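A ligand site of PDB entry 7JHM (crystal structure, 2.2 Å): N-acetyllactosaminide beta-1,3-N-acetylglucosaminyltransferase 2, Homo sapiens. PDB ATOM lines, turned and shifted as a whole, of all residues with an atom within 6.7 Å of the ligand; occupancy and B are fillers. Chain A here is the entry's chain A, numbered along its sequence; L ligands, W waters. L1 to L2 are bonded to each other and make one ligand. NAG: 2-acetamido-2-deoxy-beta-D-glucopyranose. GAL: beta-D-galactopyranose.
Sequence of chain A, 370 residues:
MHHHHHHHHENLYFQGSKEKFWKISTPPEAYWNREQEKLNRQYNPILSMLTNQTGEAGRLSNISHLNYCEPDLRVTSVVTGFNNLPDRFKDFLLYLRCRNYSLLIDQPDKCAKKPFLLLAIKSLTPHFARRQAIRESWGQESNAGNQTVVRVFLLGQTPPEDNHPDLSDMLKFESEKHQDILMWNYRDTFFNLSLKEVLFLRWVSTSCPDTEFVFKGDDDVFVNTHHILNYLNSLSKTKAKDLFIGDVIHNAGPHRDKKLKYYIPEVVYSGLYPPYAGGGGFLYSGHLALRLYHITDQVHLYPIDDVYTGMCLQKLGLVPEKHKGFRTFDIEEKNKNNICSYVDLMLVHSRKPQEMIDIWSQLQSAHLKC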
ATOM      1  N   PHE A 190     -14.674  11.727  -0.268  1.00  0.00           N
ATOM      2  CA  PHE A 190     -15.808  10.809  -0.286  1.00  0.00           C
ATOM      3  C   PHE A 190     -16.215  10.448  -1.708  1.00  0.00           C
ATOM      4  O   PHE A 190     -16.312   9.262  -2.058  1.00  0.00           O
ATOM      5  CB  PHE A 190     -16.984  11.443   0.478  1.00  0.00           C
ATOM      6  CG  PHE A 190     -18.200  10.587   0.530  1.00  0.00           C
ATOM      7  CD1 PHE A 190     -18.131   9.282   1.014  1.00  0.00           C
ATOM      8  CD2 PHE A 190     -19.439  11.092   0.140  1.00  0.00           C
ATOM      9  CE1 PHE A 190     -19.263   8.502   1.080  1.00  0.00           C
ATOM     10  CE2 PHE A 190     -20.571  10.312   0.207  1.00  0.00           C
ATOM     11  CZ  PHE A 190     -20.484   9.014   0.671  1.00  0.00           C
ATOM     12  N   ILE A 249     -27.039  -5.393  -0.633  1.00  0.00           N
ATOM     13  CA  ILE A 249     -28.248  -4.566  -0.594  1.00  0.00           C
ATOM     14  C   ILE A 249     -28.964  -4.691  -1.936  1.00  0.00           C
ATOM     15  O   ILE A 249     -28.348  -4.511  -2.994  1.00  0.00           O
ATOM     16  CB  ILE A 249     -27.900  -3.102  -0.287  1.00  0.00           C
ATOM     17  CG1 ILE A 249     -27.279  -2.983   1.105  1.00  0.00           C
ATOM     18  CG2 ILE A 249     -29.126  -2.216  -0.428  1.00  0.00           C
ATOM     19  CD1 ILE A 249     -26.280  -1.857   1.241  1.00  0.00           C
ATOM     20  N   HIS A 250     -30.252  -5.013  -1.889  1.00  0.00           N
ATOM     21  CA  HIS A 250     -31.055  -5.229  -3.087  1.00  0.00           C
ATOM     22  C   HIS A 250     -32.108  -4.135  -3.229  1.00  0.00           C
ATOM     23  O   HIS A 250     -32.731  -3.722  -2.244  1.00  0.00           O
ATOM     24  CB  HIS A 250     -31.739  -6.594  -3.053  1.00  0.00           C
ATOM     25  CG  HIS A 250     -30.853  -7.740  -3.436  1.00  0.00           C
ATOM     26  ND1 HIS A 250     -30.874  -8.309  -4.693  1.00  0.00           N
ATOM     27  CD2 HIS A 250     -29.915  -8.411  -2.729  1.00  0.00           C
ATOM     28  CE1 HIS A 250     -29.981  -9.285  -4.747  1.00  0.00           C
ATOM     29  NE2 HIS A 250     -29.385  -9.367  -3.564  1.00  0.00           N
ATOM     30  N   ASN A 251     -32.311  -3.689  -4.473  1.00  0.00           N
ATOM     31  CA  ASN A 251     -33.368  -2.742  -4.823  1.00  0.00           C
ATOM     32  C   ASN A 251     -33.244  -1.429  -4.045  1.00  0.00           C
ATOM     33  O   ASN A 251     -34.246  -0.839  -3.626  1.00  0.00           O
ATOM     34  CB  ASN A 251     -34.757  -3.348  -4.642  1.00  0.00           C
ATOM     35  CG  ASN A 251     -35.008  -4.496  -5.599  1.00  0.00           C
ATOM     36  OD1 ASN A 251     -35.304  -5.620  -5.174  1.00  0.00           O
ATOM     37  ND2 ASN A 251     -34.907  -4.226  -6.885  1.00  0.00           N
ATOM     38  N   ALA A 252     -32.018  -0.984  -3.842  1.00  0.00           N
ATOM     39  CA  ALA A 252     -31.817   0.345  -3.284  1.00  0.00           C
ATOM     40  C   ALA A 252     -31.875   1.390  -4.393  1.00  0.00           C
ATOM     41  O   ALA A 252     -31.713   1.087  -5.581  1.00  0.00           O
ATOM     42  CB  ALA A 252     -30.472   0.431  -2.561  1.00  0.00           C
ATOM     43  N   GLY A 253     -32.134   2.620  -3.989  1.00  0.00           N
ATOM     44  CA  GLY A 253     -32.130   3.736  -4.895  1.00  0.00           C
ATOM     45  C   GLY A 253     -31.346   4.901  -4.325  1.00  0.00           C
ATOM     46  O   GLY A 253     -31.029   4.930  -3.131  1.00  0.00           O
ATOM     47  N   PRO A 254     -31.006   5.868  -5.166  1.00  0.00           N
ATOM     48  CA  PRO A 254     -30.320   7.062  -4.672  1.00  0.00           C
ATOM     49  C   PRO A 254     -31.197   7.797  -3.660  1.00  0.00           C
ATOM     50  O   PRO A 254     -32.394   7.995  -3.884  1.00  0.00           O
ATOM     51  CB  PRO A 254     -30.098   7.900  -5.945  1.00  0.00           C
ATOM     52  CG  PRO A 254     -31.086   7.373  -6.935  1.00  0.00           C
ATOM     53  CD  PRO A 254     -31.199   5.906  -6.628  1.00  0.00           C
ATOM     54  N   HIS A 255     -30.590   8.169  -2.538  1.00  0.00           N
ATOM     55  CA  HIS A 255     -31.262   9.059  -1.608  1.00  0.00           C
ATOM     56  C   HIS A 255     -31.469  10.417  -2.264  1.00  0.00           C
ATOM     57  O   HIS A 255     -30.527  11.023  -2.776  1.00  0.00           O
ATOM     58  CB  HIS A 255     -30.440   9.221  -0.315  1.00  0.00           C
ATOM     59  CG  HIS A 255     -30.335   7.974   0.500  1.00  0.00           C
ATOM     60  ND1 HIS A 255     -29.167   7.262   0.626  1.00  0.00           N
ATOM     61  CD2 HIS A 255     -31.252   7.324   1.254  1.00  0.00           C
ATOM     62  CE1 HIS A 255     -29.364   6.211   1.415  1.00  0.00           C
ATOM     63  NE2 HIS A 255     -30.629   6.235   1.814  1.00  0.00           N
ATOM     64  N   TYR A 262     -25.606  10.491   1.461  1.00  0.00           N
ATOM     65  CA  TYR A 262     -25.631   9.800   0.183  1.00  0.00           C
ATOM     66  C   TYR A 262     -26.638  10.398  -0.793  1.00  0.00           C
ATOM     67  O   TYR A 262     -27.173   9.696  -1.653  1.00  0.00           O
ATOM     68  CB  TYR A 262     -25.895   8.308   0.394  1.00  0.00           C
ATOM     69  CG  TYR A 262     -24.892   7.696   1.331  1.00  0.00           C
ATOM     70  CD1 TYR A 262     -23.604   7.407   0.910  1.00  0.00           C
ATOM     71  CD2 TYR A 262     -25.231   7.426   2.652  1.00  0.00           C
ATOM     72  CE1 TYR A 262     -22.689   6.850   1.759  1.00  0.00           C
ATOM     73  CE2 TYR A 262     -24.305   6.874   3.513  1.00  0.00           C
ATOM     74  CZ  TYR A 262     -23.040   6.588   3.063  1.00  0.00           C
ATOM     75  OH  TYR A 262     -22.114   6.036   3.924  1.00  0.00           O
ATOM     76  N   TYR A 263     -26.896  11.699  -0.676  1.00  0.00           N
ATOM     77  CA  TYR A 263     -27.804  12.379  -1.581  1.00  0.00           C
ATOM     78  C   TYR A 263     -27.261  12.356  -3.010  1.00  0.00           C
ATOM     79  O   TYR A 263     -26.075  12.595  -3.249  1.00  0.00           O
ATOM     80  CB  TYR A 263     -28.002  13.816  -1.111  1.00  0.00           C
ATOM     81  CG  TYR A 263     -28.497  14.794  -2.153  1.00  0.00           C
ATOM     82  CD1 TYR A 263     -29.779  14.698  -2.666  1.00  0.00           C
ATOM     83  CD2 TYR A 263     -27.682  15.817  -2.597  1.00  0.00           C
ATOM     84  CE1 TYR A 263     -30.236  15.590  -3.618  1.00  0.00           C
ATOM     85  CE2 TYR A 263     -28.118  16.717  -3.547  1.00  0.00           C
ATOM     86  CZ  TYR A 263     -29.400  16.595  -4.050  1.00  0.00           C
ATOM     87  OH  TYR A 263     -29.836  17.495  -5.000  1.00  0.00           O
ATOM     88  N   ILE A 264     -28.140  12.022  -3.956  1.00  0.00           N
ATOM     89  CA  ILE A 264     -27.827  12.046  -5.386  1.00  0.00           C
ATOM     90  C   ILE A 264     -28.999  12.700  -6.122  1.00  0.00           C
ATOM     91  O   ILE A 264     -30.106  12.140  -6.134  1.00  0.00           O
ATOM     92  CB  ILE A 264     -27.568  10.635  -5.949  1.00  0.00           C
ATOM     93  CG1 ILE A 264     -26.461   9.917  -5.158  1.00  0.00           C
ATOM     94  CG2 ILE A 264     -27.220  10.702  -7.428  1.00  0.00           C
ATOM     95  CD1 ILE A 264     -25.064  10.425  -5.439  1.00  0.00           C
ATOM     96  N   TYR A 273     -30.363   1.222  -7.876  1.00  0.00           N
ATOM     97  CA  TYR A 273     -29.009   0.706  -7.822  1.00  0.00           C
ATOM     98  C   TYR A 273     -29.031  -0.800  -8.081  1.00  0.00           C
ATOM     99  O   TYR A 273     -29.990  -1.484  -7.713  1.00  0.00           O
ATOM    100  CB  TYR A 273     -28.378   0.990  -6.456  1.00  0.00           C
ATOM    101  CG  TYR A 273     -28.016   2.437  -6.212  1.00  0.00           C
ATOM    102  CD1 TYR A 273     -27.720   3.284  -7.269  1.00  0.00           C
ATOM    103  CD2 TYR A 273     -27.952   2.944  -4.921  1.00  0.00           C
ATOM    104  CE1 TYR A 273     -27.383   4.610  -7.045  1.00  0.00           C
ATOM    105  CE2 TYR A 273     -27.614   4.266  -4.688  1.00  0.00           C
ATOM    106  CZ  TYR A 273     -27.330   5.085  -5.756  1.00  0.00           C
ATOM    107  OH  TYR A 273     -26.994   6.406  -5.545  1.00  0.00           O
ATOM    108  N   TYR A 276     -25.499  -4.744  -4.456  1.00  0.00           N
ATOM    109  CA  TYR A 276     -24.130  -4.401  -4.115  1.00  0.00           C
ATOM    110  C   TYR A 276     -23.879  -4.668  -2.641  1.00  0.00           C
ATOM    111  O   TYR A 276     -24.774  -4.500  -1.806  1.00  0.00           O
ATOM    112  CB  TYR A 276     -23.809  -2.943  -4.457  1.00  0.00           C
ATOM    113  CG  TYR A 276     -24.493  -1.925  -3.568  1.00  0.00           C
ATOM    114  CD1 TYR A 276     -25.763  -1.460  -3.862  1.00  0.00           C
ATOM    115  CD2 TYR A 276     -23.854  -1.436  -2.440  1.00  0.00           C
ATOM    116  CE1 TYR A 276     -26.387  -0.532  -3.052  1.00  0.00           C
ATOM    117  CE2 TYR A 276     -24.466  -0.503  -1.618  1.00  0.00           C
ATOM    118  CZ  TYR A 276     -25.738  -0.053  -1.930  1.00  0.00           C
ATOM    119  OH  TYR A 276     -26.351   0.876  -1.120  1.00  0.00           O
ATOM    120  N   ALA A 277     -22.658  -5.077  -2.339  1.00  0.00           N
ATOM    121  CA  ALA A 277     -22.234  -5.270  -0.958  1.00  0.00           C
ATOM    122  C   ALA A 277     -21.855  -3.923  -0.343  1.00  0.00           C
ATOM    123  O   ALA A 277     -21.184  -3.103  -0.974  1.00  0.00           O
ATOM    124  CB  ALA A 277     -21.047  -6.230  -0.890  1.00  0.00           C
ATOM    125  N   GLY A 278     -22.284  -3.716   0.905  1.00  0.00           N
ATOM    126  CA  GLY A 278     -21.898  -2.509   1.610  1.00  0.00           C
ATOM    127  C   GLY A 278     -20.389  -2.390   1.693  1.00  0.00           C
ATOM    128  O   GLY A 278     -19.675  -3.359   1.946  1.00  0.00           O
ATOM    129  N   GLY A 279     -19.897  -1.165   1.483  1.00  0.00           N
ATOM    130  CA  GLY A 279     -18.464  -0.909   1.392  1.00  0.00           C
ATOM    131  C   GLY A 279     -17.698  -1.073   2.686  1.00  0.00           C
ATOM    132  O   GLY A 279     -16.463  -1.005   2.652  1.00  0.00           O
ATOM    133  N   GLY A 280     -18.377  -1.280   3.816  1.00  0.00           N
ATOM    134  CA  GLY A 280     -17.678  -1.527   5.057  1.00  0.00           C
ATOM    135  C   GLY A 280     -16.692  -2.676   4.960  1.00  0.00           C
ATOM    136  O   GLY A 280     -15.647  -2.660   5.614  1.00  0.00           O
ATOM    137  N   ILE A 304     -20.698   6.959  -5.347  1.00  0.00           N
ATOM    138  CA  ILE A 304     -20.766   6.032  -4.216  1.00  0.00           C
ATOM    139  C   ILE A 304     -19.973   4.784  -4.604  1.00  0.00           C
ATOM    140  O   ILE A 304     -20.346   4.076  -5.548  1.00  0.00           O
ATOM    141  CB  ILE A 304     -22.212   5.677  -3.851  1.00  0.00           C
ATOM    142  CG1 ILE A 304     -23.080   6.934  -3.793  1.00  0.00           C
ATOM    143  CG2 ILE A 304     -22.246   4.955  -2.521  1.00  0.00           C
ATOM    144  CD1 ILE A 304     -22.553   8.015  -2.872  1.00  0.00           C
ATOM    145  N   ASP A 305     -18.895   4.507  -3.865  1.00  0.00           N
ATOM    146  CA  ASP A 305     -17.944   3.499  -4.324  1.00  0.00           C
ATOM    147  C   ASP A 305     -18.503   2.073  -4.241  1.00  0.00           C
ATOM    148  O   ASP A 305     -18.185   1.253  -5.105  1.00  0.00           O
ATOM    149  CB  ASP A 305     -16.633   3.602  -3.535  1.00  0.00           C
ATOM    150  CG  ASP A 305     -16.788   3.237  -2.077  1.00  0.00           C
ATOM    151  OD1 ASP A 305     -17.848   3.530  -1.500  1.00  0.00           O
ATOM    152  OD2 ASP A 305     -15.833   2.672  -1.510  1.00  0.00           O
ATOM    153  N   ASP A 306     -19.318   1.754  -3.237  1.00  0.00           N
ATOM    154  CA  ASP A 306     -19.809   0.371  -3.186  1.00  0.00           C
ATOM    155  C   ASP A 306     -20.897   0.111  -4.222  1.00  0.00           C
ATOM    156  O   ASP A 306     -21.035  -1.026  -4.677  1.00  0.00           O
ATOM    157  CB  ASP A 306     -20.279  -0.001  -1.766  1.00  0.00           C
ATOM    158  CG  ASP A 306     -21.170   1.044  -1.130  1.00  0.00           C
ATOM    159  OD1 ASP A 306     -21.416   0.934   0.088  1.00  0.00           O
ATOM    160  OD2 ASP A 306     -21.631   1.969  -1.836  1.00  0.00           O
ATOM    161  N   VAL A 307     -21.656   1.138  -4.621  1.00  0.00           N
ATOM    162  CA  VAL A 307     -22.552   0.988  -5.757  1.00  0.00           C
ATOM    163  C   VAL A 307     -21.754   0.758  -7.029  1.00  0.00           C
ATOM    164  O   VAL A 307     -22.119  -0.071  -7.875  1.00  0.00           O
ATOM    165  CB  VAL A 307     -23.470   2.221  -5.883  1.00  0.00           C
ATOM    166  CG1 VAL A 307     -24.252   2.187  -7.199  1.00  0.00           C
ATOM    167  CG2 VAL A 307     -24.419   2.288  -4.692  1.00  0.00           C
ATOM    168  N   THR A 328     -22.703  -4.904   8.880  1.00  0.00           N
ATOM    169  CA  THR A 328     -22.330  -3.529   8.572  1.00  0.00           C
ATOM    170  C   THR A 328     -23.194  -2.495   9.277  1.00  0.00           C
ATOM    171  O   THR A 328     -22.972  -1.297   9.091  1.00  0.00           O
ATOM    172  CB  THR A 328     -22.376  -3.308   7.046  1.00  0.00           C
ATOM    173  OG1 THR A 328     -23.689  -3.590   6.562  1.00  0.00           O
ATOM    174  CG2 THR A 328     -21.378  -4.205   6.357  1.00  0.00           C
ATOM    175  N   PHE A 329     -24.173  -2.922  10.082  1.00  0.00           N
ATOM    176  CA  PHE A 329     -24.943  -2.035  10.933  1.00  0.00           C
ATOM    177  C   PHE A 329     -24.942  -2.542  12.367  1.00  0.00           C
ATOM    178  O   PHE A 329     -25.819  -2.215  13.161  1.00  0.00           O
ATOM    179  CB  PHE A 329     -26.374  -1.838  10.400  1.00  0.00           C
ATOM    180  CG  PHE A 329     -26.438  -1.385   8.948  1.00  0.00           C
ATOM    181  CD1 PHE A 329     -26.812  -0.087   8.623  1.00  0.00           C
ATOM    182  CD2 PHE A 329     -26.149  -2.270   7.915  1.00  0.00           C
ATOM    183  CE1 PHE A 329     -26.875   0.322   7.294  1.00  0.00           C
ATOM    184  CE2 PHE A 329     -26.201  -1.852   6.588  1.00  0.00           C
ATOM    185  CZ  PHE A 329     -26.564  -0.559   6.271  1.00  0.00           C
HETATM  186  C1  NAG L   1     -30.655   0.862   3.764  1.00  0.00           C
HETATM  187  C2  NAG L   1     -30.758   1.179   2.254  1.00  0.00           C
HETATM  188  C3  NAG L   1     -29.295   1.223   1.724  1.00  0.00           C
HETATM  189  C4  NAG L   1     -28.387   2.187   2.555  1.00  0.00           C
HETATM  190  C5  NAG L   1     -28.687   2.079   4.122  1.00  0.00           C
HETATM  191  C6  NAG L   1     -28.161   3.391   4.795  1.00  0.00           C
HETATM  192  C7  NAG L   1     -32.384   0.340   0.503  1.00  0.00           C
HETATM  193  C8  NAG L   1     -33.021  -0.887  -0.099  1.00  0.00           C
HETATM  194  N2  NAG L   1     -31.465   0.118   1.536  1.00  0.00           N
HETATM  195  O1  NAG L   1     -31.964   0.880   4.230  1.00  0.00           O
HETATM  196  O3  NAG L   1     -29.225   1.675   0.401  1.00  0.00           O
HETATM  197  O4  NAG L   1     -27.057   1.773   2.360  1.00  0.00           O
HETATM  198  O5  NAG L   1     -30.058   1.960   4.389  1.00  0.00           O
HETATM  199  O6  NAG L   1     -28.540   4.515   4.073  1.00  0.00           O
HETATM  200  O7  NAG L   1     -32.637   1.473   0.114  1.00  0.00           O
HETATM  201  C1  GAL L   2     -26.099   2.772   2.123  1.00  0.00           C
HETATM  202  C2  GAL L   2     -24.677   2.182   2.159  1.00  0.00           C
HETATM  203  C3  GAL L   2     -23.655   3.272   1.857  1.00  0.00           C
HETATM  204  C4  GAL L   2     -24.001   3.879   0.469  1.00  0.00           C
HETATM  205  C5  GAL L   2     -25.482   4.332   0.377  1.00  0.00           C
HETATM  206  C6  GAL L   2     -25.897   4.719  -1.049  1.00  0.00           C
HETATM  207  O2  GAL L   2     -24.494   1.785   3.493  1.00  0.00           O
HETATM  208  O3  GAL L   2     -22.426   2.635   1.880  1.00  0.00           O
HETATM  209  O4  GAL L   2     -23.763   2.847  -0.450  1.00  0.00           O
HETATM  210  O5  GAL L   2     -26.368   3.376   0.902  1.00  0.00           O
HETATM  211  O6  GAL L   2     -27.131   5.388  -0.947  1.00  0.00           O
HETATM  212  O   HOH W   1     -27.411   7.191  -3.036  1.00  0.00           O
HETATM  213  O   HOH W   2     -29.089   3.606  -1.197  1.00  0.00           O
HETATM  214  O   HOH W   3     -20.118   2.199   3.441  1.00  0.00           O
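Residues that only touch the ligand: Ile 249, His 250, Asn 251, Ala 252, Tyr 262, Tyr 273 and Ile 304. Hydrophobic or aromatic side chains within 4 Å of the ligand: Ile 249, Ala 252, His 255, Tyr 262, Tyr 273, Tyr 276 and Ile 304. Ten residues have an atom within 4 Å of the ligand: Ile 249, His 250, Asn 251, Ala 252, His 255, Tyr 262, Tyr 273, Tyr 276, Ile 304 and Asp 306. The nearest printed residue that does not touch the ligand is Phe 329 (4.01 Å).
Water W2 lies within hydrogen-bond range of O3 of NAG L1 (2.5 Å) and O of Gly 253 (3.0 Å). Water W1 lies within hydrogen-bond range of the side-chain hydroxyl (OH) of Tyr 273 (2.7 Å), an oxygen (O6) of GAL L2 (2.8 Å), the backbone carbonyl oxygen (O) of Tyr 262 (2.9 Å) and the backbone NH (N) of His 255 (3.4 Å).
The backbone carbonyl oxygen (O) of Tyr 276 sits at hydrogen-bond distance from the backbone NH (N) of Ile 249. N of Gly 279 lies within hydrogen-bond range of OD1 of Asp 306. The backbone carbonyl oxygen (O) of His 255 lies within hydrogen-bond range of the backbone NH (N) of Ile 264. The backbone carbonyl oxygen of Ala 252 is in hydrogen-bond range of the backbone NH of Tyr 273.
A ring nitrogen (ND1) of His 255 is in hydrogen-bond range of an oxygen (O6) of GAL L2, at 3.2 Å. OD1 of Asp 306 sits at hydrogen-bond distance from O3 of GAL L2, 2.7 Å away. The side-chain hydroxyl of Tyr 276 sits at hydrogen-bond distance from an oxygen (O5) of GAL L2.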
